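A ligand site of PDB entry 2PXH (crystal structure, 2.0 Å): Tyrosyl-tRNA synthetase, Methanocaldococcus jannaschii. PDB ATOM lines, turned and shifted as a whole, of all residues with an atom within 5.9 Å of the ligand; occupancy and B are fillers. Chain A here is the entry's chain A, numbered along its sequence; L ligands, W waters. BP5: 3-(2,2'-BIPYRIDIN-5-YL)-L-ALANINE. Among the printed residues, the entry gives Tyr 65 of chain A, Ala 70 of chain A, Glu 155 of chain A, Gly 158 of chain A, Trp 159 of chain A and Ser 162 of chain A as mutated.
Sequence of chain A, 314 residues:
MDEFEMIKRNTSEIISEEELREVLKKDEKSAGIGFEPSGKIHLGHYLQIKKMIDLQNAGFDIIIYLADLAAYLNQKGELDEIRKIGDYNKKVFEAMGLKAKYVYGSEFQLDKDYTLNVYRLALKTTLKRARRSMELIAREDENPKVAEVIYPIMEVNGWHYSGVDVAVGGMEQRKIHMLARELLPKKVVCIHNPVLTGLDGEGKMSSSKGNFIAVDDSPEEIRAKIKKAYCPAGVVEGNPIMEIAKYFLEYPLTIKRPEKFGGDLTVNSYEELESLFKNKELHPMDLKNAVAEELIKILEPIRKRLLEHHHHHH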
ATOM      1  N   ILE A  33       2.551 -19.096  25.588  1.00  0.00           N
ATOM      2  CA  ILE A  33       3.379 -19.515  26.724  1.00  0.00           C
ATOM      3  C   ILE A  33       2.370 -19.688  27.838  1.00  0.00           C
ATOM      4  O   ILE A  33       1.331 -19.069  27.810  1.00  0.00           O
ATOM      5  CB  ILE A  33       4.495 -18.432  27.065  1.00  0.00           C
ATOM      6  CG1 ILE A  33       5.394 -18.871  28.235  1.00  0.00           C
ATOM      7  CG2 ILE A  33       3.902 -17.046  27.341  1.00  0.00           C
ATOM      8  CD1 ILE A  33       6.776 -18.202  28.176  1.00  0.00           C
ATOM      9  N   GLY A  34       2.657 -20.515  28.825  1.00  0.00           N
ATOM     10  CA  GLY A  34       1.822 -20.539  29.992  1.00  0.00           C
ATOM     11  C   GLY A  34       2.672 -20.529  31.216  1.00  0.00           C
ATOM     12  O   GLY A  34       3.822 -20.990  31.194  1.00  0.00           O
ATOM     13  N   PHE A  35       2.115 -20.012  32.299  1.00  0.00           N
ATOM     14  CA  PHE A  35       2.822 -19.942  33.553  1.00  0.00           C
ATOM     15  C   PHE A  35       1.854 -20.464  34.600  1.00  0.00           C
ATOM     16  O   PHE A  35       0.684 -20.033  34.662  1.00  0.00           O
ATOM     17  CB  PHE A  35       3.141 -18.454  33.891  1.00  0.00           C
ATOM     18  CG  PHE A  35       4.033 -17.744  32.883  1.00  0.00           C
ATOM     19  CD1 PHE A  35       3.510 -16.808  32.015  1.00  0.00           C
ATOM     20  CD2 PHE A  35       5.392 -17.996  32.872  1.00  0.00           C
ATOM     21  CE1 PHE A  35       4.354 -16.128  31.106  1.00  0.00           C
ATOM     22  CE2 PHE A  35       6.252 -17.307  32.010  1.00  0.00           C
ATOM     23  CZ  PHE A  35       5.730 -16.391  31.131  1.00  0.00           C
ATOM     24  N   GLU A  36       2.336 -21.356  35.460  1.00  0.00           N
ATOM     25  CA  GLU A  36       1.641 -21.604  36.724  1.00  0.00           C
ATOM     26  C   GLU A  36       1.680 -20.276  37.495  1.00  0.00           C
ATOM     27  O   GLU A  36       2.769 -19.693  37.613  1.00  0.00           O
ATOM     28  CB  GLU A  36       2.413 -22.688  37.471  1.00  0.00           C
ATOM     29  CG  GLU A  36       2.351 -24.073  36.810  1.00  0.00           C
ATOM     30  CD  GLU A  36       3.046 -25.071  37.684  1.00  0.00           C
ATOM     31  OE1 GLU A  36       2.833 -24.982  38.900  1.00  0.00           O
ATOM     32  OE2 GLU A  36       3.741 -25.970  37.181  1.00  0.00           O
ATOM     33  N   TYR A  65      -1.216 -18.340  28.742  1.00  0.00           N
ATOM     34  CA  TYR A  65      -2.071 -19.193  29.545  1.00  0.00           C
ATOM     35  C   TYR A  65      -1.744 -18.979  30.982  1.00  0.00           C
ATOM     36  O   TYR A  65      -0.624 -19.172  31.390  1.00  0.00           O
ATOM     37  CB  TYR A  65      -1.962 -20.663  29.121  1.00  0.00           C
ATOM     38  CG  TYR A  65      -2.559 -20.833  27.742  1.00  0.00           C
ATOM     39  CD1 TYR A  65      -1.749 -20.875  26.621  1.00  0.00           C
ATOM     40  CD2 TYR A  65      -3.961 -20.943  27.578  1.00  0.00           C
ATOM     41  CE1 TYR A  65      -2.293 -21.007  25.353  1.00  0.00           C
ATOM     42  CE2 TYR A  65      -4.525 -21.099  26.304  1.00  0.00           C
ATOM     43  CZ  TYR A  65      -3.676 -21.133  25.209  1.00  0.00           C
ATOM     44  OH  TYR A  65      -4.221 -21.278  23.945  1.00  0.00           O
ATOM     45  N   ALA A  67      -1.889 -20.709  33.815  1.00  0.00           N
ATOM     46  CA  ALA A  67      -2.086 -22.169  33.857  1.00  0.00           C
ATOM     47  C   ALA A  67      -2.605 -22.589  35.222  1.00  0.00           C
ATOM     48  O   ALA A  67      -1.903 -23.216  35.999  1.00  0.00           O
ATOM     49  CB  ALA A  67      -0.820 -22.895  33.481  1.00  0.00           C
ATOM     50  N   ALA A  70      -2.856 -26.529  35.719  1.00  0.00           N
ATOM     51  CA  ALA A  70      -1.505 -27.068  35.853  1.00  0.00           C
ATOM     52  C   ALA A  70      -0.976 -26.816  37.243  1.00  0.00           C
ATOM     53  O   ALA A  70      -0.295 -27.657  37.823  1.00  0.00           O
ATOM     54  CB  ALA A  70      -0.561 -26.361  34.859  1.00  0.00           C
ATOM     55  N   GLY A 105      -6.351 -21.781  31.862  1.00  0.00           N
ATOM     56  CA  GLY A 105      -6.482 -23.098  31.219  1.00  0.00           C
ATOM     57  C   GLY A 105      -7.815 -23.780  31.603  1.00  0.00           C
ATOM     58  O   GLY A 105      -8.470 -24.394  30.762  1.00  0.00           O
ATOM     59  N   PHE A 108     -11.130 -24.142  29.562  1.00  0.00           N
ATOM     60  CA  PHE A 108     -11.419 -25.184  28.542  1.00  0.00           C
ATOM     61  C   PHE A 108     -10.899 -26.592  28.889  1.00  0.00           C
ATOM     62  O   PHE A 108     -11.275 -27.563  28.271  1.00  0.00           O
ATOM     63  CB  PHE A 108     -10.911 -24.744  27.168  1.00  0.00           C
ATOM     64  CG  PHE A 108      -9.418 -24.509  27.125  1.00  0.00           C
ATOM     65  CD1 PHE A 108      -8.526 -25.559  26.823  1.00  0.00           C
ATOM     66  CD2 PHE A 108      -8.897 -23.266  27.402  1.00  0.00           C
ATOM     67  CE1 PHE A 108      -7.144 -25.357  26.779  1.00  0.00           C
ATOM     68  CE2 PHE A 108      -7.497 -23.062  27.390  1.00  0.00           C
ATOM     69  CZ  PHE A 108      -6.619 -24.120  27.065  1.00  0.00           C
ATOM     70  N   GLN A 109     -10.016 -26.707  29.872  1.00  0.00           N
ATOM     71  CA  GLN A 109      -9.284 -27.928  30.108  1.00  0.00           C
ATOM     72  C   GLN A 109     -10.088 -28.950  30.904  1.00  0.00           C
ATOM     73  O   GLN A 109      -9.535 -29.970  31.288  1.00  0.00           O
ATOM     74  CB  GLN A 109      -7.952 -27.635  30.840  1.00  0.00           C
ATOM     75  CG  GLN A 109      -6.853 -27.019  29.940  1.00  0.00           C
ATOM     76  CD  GLN A 109      -5.534 -26.793  30.652  1.00  0.00           C
ATOM     77  OE1 GLN A 109      -5.493 -26.256  31.753  1.00  0.00           O
ATOM     78  NE2 GLN A 109      -4.456 -27.173  30.012  1.00  0.00           N
ATOM     79  N   TYR A 114     -12.302 -32.362  25.771  1.00  0.00           N
ATOM     80  CA  TYR A 114     -10.893 -32.132  26.122  1.00  0.00           C
ATOM     81  C   TYR A 114     -10.371 -33.298  27.018  1.00  0.00           C
ATOM     82  O   TYR A 114      -9.296 -33.844  26.795  1.00  0.00           O
ATOM     83  CB  TYR A 114     -10.769 -30.810  26.905  1.00  0.00           C
ATOM     84  CG  TYR A 114      -9.329 -30.439  27.214  1.00  0.00           C
ATOM     85  CD1 TYR A 114      -8.631 -29.521  26.412  1.00  0.00           C
ATOM     86  CD2 TYR A 114      -8.659 -31.005  28.305  1.00  0.00           C
ATOM     87  CE1 TYR A 114      -7.305 -29.180  26.712  1.00  0.00           C
ATOM     88  CE2 TYR A 114      -7.330 -30.670  28.589  1.00  0.00           C
ATOM     89  CZ  TYR A 114      -6.669 -29.759  27.785  1.00  0.00           C
ATOM     90  OH  TYR A 114      -5.377 -29.431  28.068  1.00  0.00           O
ATOM     91  N   ILE A 137      10.181 -29.490  36.670  1.00  0.00           N
ATOM     92  CA  ILE A 137       8.931 -28.739  36.822  1.00  0.00           C
ATOM     93  C   ILE A 137       8.145 -29.138  38.037  1.00  0.00           C
ATOM     94  O   ILE A 137       7.541 -28.278  38.688  1.00  0.00           O
ATOM     95  CB  ILE A 137       8.054 -28.910  35.567  1.00  0.00           C
ATOM     96  CG1 ILE A 137       8.726 -28.131  34.417  1.00  0.00           C
ATOM     97  CG2 ILE A 137       6.597 -28.403  35.796  1.00  0.00           C
ATOM     98  CD1 ILE A 137       8.411 -28.684  33.124  1.00  0.00           C
ATOM     99  N   TYR A 151      -0.100 -33.877  34.682  1.00  0.00           N
ATOM    100  CA  TYR A 151       0.360 -32.523  34.281  1.00  0.00           C
ATOM    101  C   TYR A 151       0.924 -32.430  32.848  1.00  0.00           C
ATOM    102  O   TYR A 151       0.423 -31.612  32.050  1.00  0.00           O
ATOM    103  CB  TYR A 151       1.359 -32.045  35.334  1.00  0.00           C
ATOM    104  CG  TYR A 151       1.876 -30.643  35.158  1.00  0.00           C
ATOM    105  CD1 TYR A 151       1.604 -29.681  36.100  1.00  0.00           C
ATOM    106  CD2 TYR A 151       2.726 -30.325  34.078  1.00  0.00           C
ATOM    107  CE1 TYR A 151       2.130 -28.378  35.960  1.00  0.00           C
ATOM    108  CE2 TYR A 151       3.250 -29.050  33.923  1.00  0.00           C
ATOM    109  CZ  TYR A 151       2.945 -28.086  34.867  1.00  0.00           C
ATOM    110  OH  TYR A 151       3.478 -26.831  34.783  1.00  0.00           O
ATOM    111  N   MET A 154      -1.870 -33.060  30.353  1.00  0.00           N
ATOM    112  CA  MET A 154      -2.753 -31.871  30.414  1.00  0.00           C
ATOM    113  C   MET A 154      -2.197 -30.723  29.531  1.00  0.00           C
ATOM    114  O   MET A 154      -2.923 -30.075  28.787  1.00  0.00           O
ATOM    115  CB  MET A 154      -2.932 -31.396  31.870  1.00  0.00           C
ATOM    116  CG  MET A 154      -3.659 -30.079  32.027  1.00  0.00           C
ATOM    117  SD  MET A 154      -5.339 -30.239  31.410  1.00  0.00           S
ATOM    118  CE  MET A 154      -5.971 -31.605  32.369  1.00  0.00           C
ATOM    119  N   GLU A 155      -0.911 -30.453  29.649  1.00  0.00           N
ATOM    120  CA  GLU A 155      -0.310 -29.331  28.929  1.00  0.00           C
ATOM    121  C   GLU A 155      -0.194 -29.662  27.469  1.00  0.00           C
ATOM    122  O   GLU A 155      -0.425 -28.809  26.645  1.00  0.00           O
ATOM    123  CB  GLU A 155       1.112 -29.057  29.444  1.00  0.00           C
ATOM    124  CG  GLU A 155       1.782 -27.958  28.622  1.00  0.00           C
ATOM    125  CD  GLU A 155       3.074 -27.380  29.204  1.00  0.00           C
ATOM    126  OE1 GLU A 155       3.289 -27.463  30.432  1.00  0.00           O
ATOM    127  OE2 GLU A 155       3.833 -26.778  28.406  1.00  0.00           O
ATOM    128  N   ASN A 157      -2.112 -31.630  25.670  1.00  0.00           N
ATOM    129  CA  ASN A 157      -3.426 -31.402  25.115  1.00  0.00           C
ATOM    130  C   ASN A 157      -3.747 -29.932  25.040  1.00  0.00           C
ATOM    131  O   ASN A 157      -4.465 -29.487  24.129  1.00  0.00           O
ATOM    132  CB  ASN A 157      -4.510 -32.156  25.943  1.00  0.00           C
ATOM    133  CG  ASN A 157      -5.758 -32.457  25.112  1.00  0.00           C
ATOM    134  OD1 ASN A 157      -5.682 -32.708  23.896  1.00  0.00           O
ATOM    135  ND2 ASN A 157      -6.911 -32.455  25.763  1.00  0.00           N
ATOM    136  N   GLY A 158      -3.261 -29.139  25.988  1.00  0.00           N
ATOM    137  CA  GLY A 158      -3.453 -27.670  25.897  1.00  0.00           C
ATOM    138  C   GLY A 158      -2.824 -27.109  24.642  1.00  0.00           C
ATOM    139  O   GLY A 158      -3.438 -26.293  23.937  1.00  0.00           O
ATOM    140  N   TRP A 159      -1.577 -27.507  24.362  1.00  0.00           N
ATOM    141  CA  TRP A 159      -0.943 -27.022  23.147  1.00  0.00           C
ATOM    142  C   TRP A 159      -1.754 -27.399  21.906  1.00  0.00           C
ATOM    143  O   TRP A 159      -1.850 -26.618  20.976  1.00  0.00           O
ATOM    144  CB  TRP A 159       0.512 -27.527  23.003  1.00  0.00           C
ATOM    145  CG  TRP A 159       1.433 -26.908  24.046  1.00  0.00           C
ATOM    146  CD1 TRP A 159       2.111 -27.565  25.010  1.00  0.00           C
ATOM    147  CD2 TRP A 159       1.775 -25.523  24.182  1.00  0.00           C
ATOM    148  NE1 TRP A 159       2.849 -26.690  25.747  1.00  0.00           N
ATOM    149  CE2 TRP A 159       2.651 -25.416  25.282  1.00  0.00           C
ATOM    150  CE3 TRP A 159       1.406 -24.355  23.495  1.00  0.00           C
ATOM    151  CZ2 TRP A 159       3.191 -24.181  25.730  1.00  0.00           C
ATOM    152  CZ3 TRP A 159       1.924 -23.105  23.960  1.00  0.00           C
ATOM    153  CH2 TRP A 159       2.817 -23.047  25.048  1.00  0.00           C
ATOM    154  N   SER A 162      -4.732 -25.133  21.812  1.00  0.00           N
ATOM    155  CA  SER A 162      -4.402 -23.714  21.645  1.00  0.00           C
ATOM    156  C   SER A 162      -4.357 -23.327  20.194  1.00  0.00           C
ATOM    157  O   SER A 162      -4.556 -22.150  19.856  1.00  0.00           O
ATOM    158  CB  SER A 162      -3.049 -23.386  22.268  1.00  0.00           C
ATOM    159  OG  SER A 162      -2.000 -23.955  21.495  1.00  0.00           O
ATOM    160  N   GLU A 172      13.739 -25.598  30.746  1.00  0.00           N
ATOM    161  CA  GLU A 172      13.222 -26.679  31.566  1.00  0.00           C
ATOM    162  C   GLU A 172      11.927 -27.265  31.006  1.00  0.00           C
ATOM    163  O   GLU A 172      11.567 -28.400  31.333  1.00  0.00           O
ATOM    164  CB  GLU A 172      13.061 -26.233  33.048  1.00  0.00           C
ATOM    165  CG  GLU A 172      11.811 -25.406  33.414  1.00  0.00           C
ATOM    166  CD  GLU A 172      11.791 -23.970  32.848  1.00  0.00           C
ATOM    167  OE1 GLU A 172      12.819 -23.363  32.481  1.00  0.00           O
ATOM    168  OE2 GLU A 172      10.696 -23.401  32.776  1.00  0.00           O
ATOM    169  N   GLN A 173      11.252 -26.492  30.155  1.00  0.00           N
ATOM    170  CA  GLN A 173      10.028 -26.955  29.502  1.00  0.00           C
ATOM    171  C   GLN A 173      10.316 -27.905  28.366  1.00  0.00           C
ATOM    172  O   GLN A 173       9.403 -28.426  27.764  1.00  0.00           O
ATOM    173  CB  GLN A 173       9.225 -25.759  28.940  1.00  0.00           C
ATOM    174  CG  GLN A 173       8.867 -24.673  29.951  1.00  0.00           C
ATOM    175  CD  GLN A 173       8.051 -25.174  31.107  1.00  0.00           C
ATOM    176  OE1 GLN A 173       6.969 -25.781  30.925  1.00  0.00           O
ATOM    177  NE2 GLN A 173       8.547 -24.964  32.317  1.00  0.00           N
ATOM    178  N   ILE A 176       8.538 -31.562  28.047  1.00  0.00           N
ATOM    179  CA  ILE A 176       7.075 -31.482  27.820  1.00  0.00           C
ATOM    180  C   ILE A 176       6.816 -31.072  26.369  1.00  0.00           C
ATOM    181  O   ILE A 176       5.946 -31.610  25.680  1.00  0.00           O
ATOM    182  CB  ILE A 176       6.365 -30.511  28.795  1.00  0.00           C
ATOM    183  CG1 ILE A 176       6.342 -31.105  30.217  1.00  0.00           C
ATOM    184  CG2 ILE A 176       4.902 -30.292  28.331  1.00  0.00           C
ATOM    185  CD1 ILE A 176       5.671 -30.184  31.246  1.00  0.00           C
HETATM  186  C9  BP5 L   1       2.203 -24.465  31.352  1.00  0.00           C
HETATM  187  C8  BP5 L   1       2.551 -23.919  30.114  1.00  0.00           C
HETATM  188  C7  BP5 L   1       1.591 -24.013  29.068  1.00  0.00           C
HETATM  189  C6  BP5 L   1       0.346 -24.669  29.298  1.00  0.00           C
HETATM  190  C5  BP5 L   1      -2.735 -24.374  26.553  1.00  0.00           C
HETATM  191  C4  BP5 L   1      -2.921 -24.505  27.913  1.00  0.00           C
HETATM  192  C3  BP5 L   1      -0.627 -24.656  28.317  1.00  0.00           C
HETATM  193  C2  BP5 L   1      -0.387 -24.477  26.952  1.00  0.00           C
HETATM  194  C1  BP5 L   1      -1.440 -24.335  26.051  1.00  0.00           C
HETATM  195  C12 BP5 L   1       3.141 -24.372  32.625  1.00  0.00           C
HETATM  196  C11 BP5 L   1       0.947 -25.069  31.519  1.00  0.00           C
HETATM  197  N1  BP5 L   1      -1.888 -24.632  28.769  1.00  0.00           N
HETATM  198  N2  BP5 L   1       0.033 -25.162  30.540  1.00  0.00           N
HETATM  199  CA  BP5 L   1       4.608 -24.603  32.389  1.00  0.00           C
HETATM  200  C   BP5 L   1       5.358 -24.127  33.649  1.00  0.00           C
HETATM  201  OXT BP5 L   1       6.164 -24.932  34.212  1.00  0.00           O
HETATM  202  O   BP5 L   1       5.082 -22.973  34.058  1.00  0.00           O
HETATM  203  N   BP5 L   1       4.710 -26.067  32.214  1.00  0.00           N
HETATM  204  O   HOH W   1      -3.146 -23.412  31.024  1.00  0.00           O
HETATM  205  O   HOH W   2       5.570 -25.029  28.744  1.00  0.00           O
HETATM  206  O   HOH W   3       7.421 -24.436  36.425  1.00  0.00           O
HETATM  207  O   HOH W   4      -1.922 -27.085  31.562  1.00  0.00           O
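N of the ligand sits at hydrogen-bond distance from OE1 of Gln 173 (2.6 Å).
N of the ligand sits at hydrogen-bond distance from OH of Tyr 151.
OE1 of Glu 155 is in salt-bridge range of N of the ligand (2.7 Å).
An oxygen (O) of the ligand sits at hydrogen-bond distance from the backbone NH (N) of Glu 36, 3.5 Å away.
The side-chain carboxylate of Glu 155 is in hydrogen-bond range of the indole nitrogen of Trp 159 (2.8 Å).
The side-chain amide nitrogen (NE2) of Gln 173 lies within hydrogen-bond range of the side-chain carboxylate (OE2) of Glu 172 (2.7 Å).
The backbone carbonyl oxygen of Trp 159 lies within hydrogen-bond range of the side-chain hydroxyl of Ser 162 (2.7 Å).
The backbone NH (N) of Ala 67 is in hydrogen-bond range of the backbone carbonyl oxygen (O) of Phe 35, 2.8 Å away.
The backbone carbonyl oxygen (O) of Tyr 65 is in hydrogen-bond range of the backbone NH (N) of Phe 35.
The backbone carbonyl oxygen of Ile 33 sits at hydrogen-bond distance from the backbone NH of Tyr 65 (2.8 Å).
The side-chain amide nitrogen of Gln 109 is in hydrogen-bond range of the side-chain hydroxyl of Tyr 114 (3.1 Å).
The side-chain hydroxyl of Tyr 151 lies within hydrogen-bond range of the side-chain carboxylate of Glu 36 (2.6 Å).
Residues that only touch the ligand: Gly 158 (3.3 Å), Gly 34 (3.4 Å), Ala 67 (3.4 Å), Tyr 65 (3.5 Å), Trp 159 (3.6 Å), Gln 109 (3.7 Å), Phe 108 (3.8 Å), Phe 35 (3.8 Å), Ile 137 (3.8 Å) and Ala 70 (3.9 Å).
Hydrophobic or aromatic side chains within 4 Å of the ligand: Tyr 65, Ala 67, Ala 70, Phe 108, Ile 137, Tyr 151 and Trp 159.
14 residues have an atom within 4 Å of the ligand: Gly 34, Phe 35, Glu 36, Tyr 65, Ala 67, Ala 70, Phe 108, Gln 109, Ile 137, Tyr 151, Glu 155, Gly 158, Trp 159 and Gln 173.
Along chain A the residues within 4 Å of the ligand span positions 34 to 173.
Water W4 lies within hydrogen-bond range of a nitrogen (N2) of the ligand and the side-chain amide nitrogen of Gln 109.
Water W2 bridges the side-chain carboxylate of Glu 155 (2.5 Å) and the side-chain amide oxygen of Gln 173 (2.7 Å).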
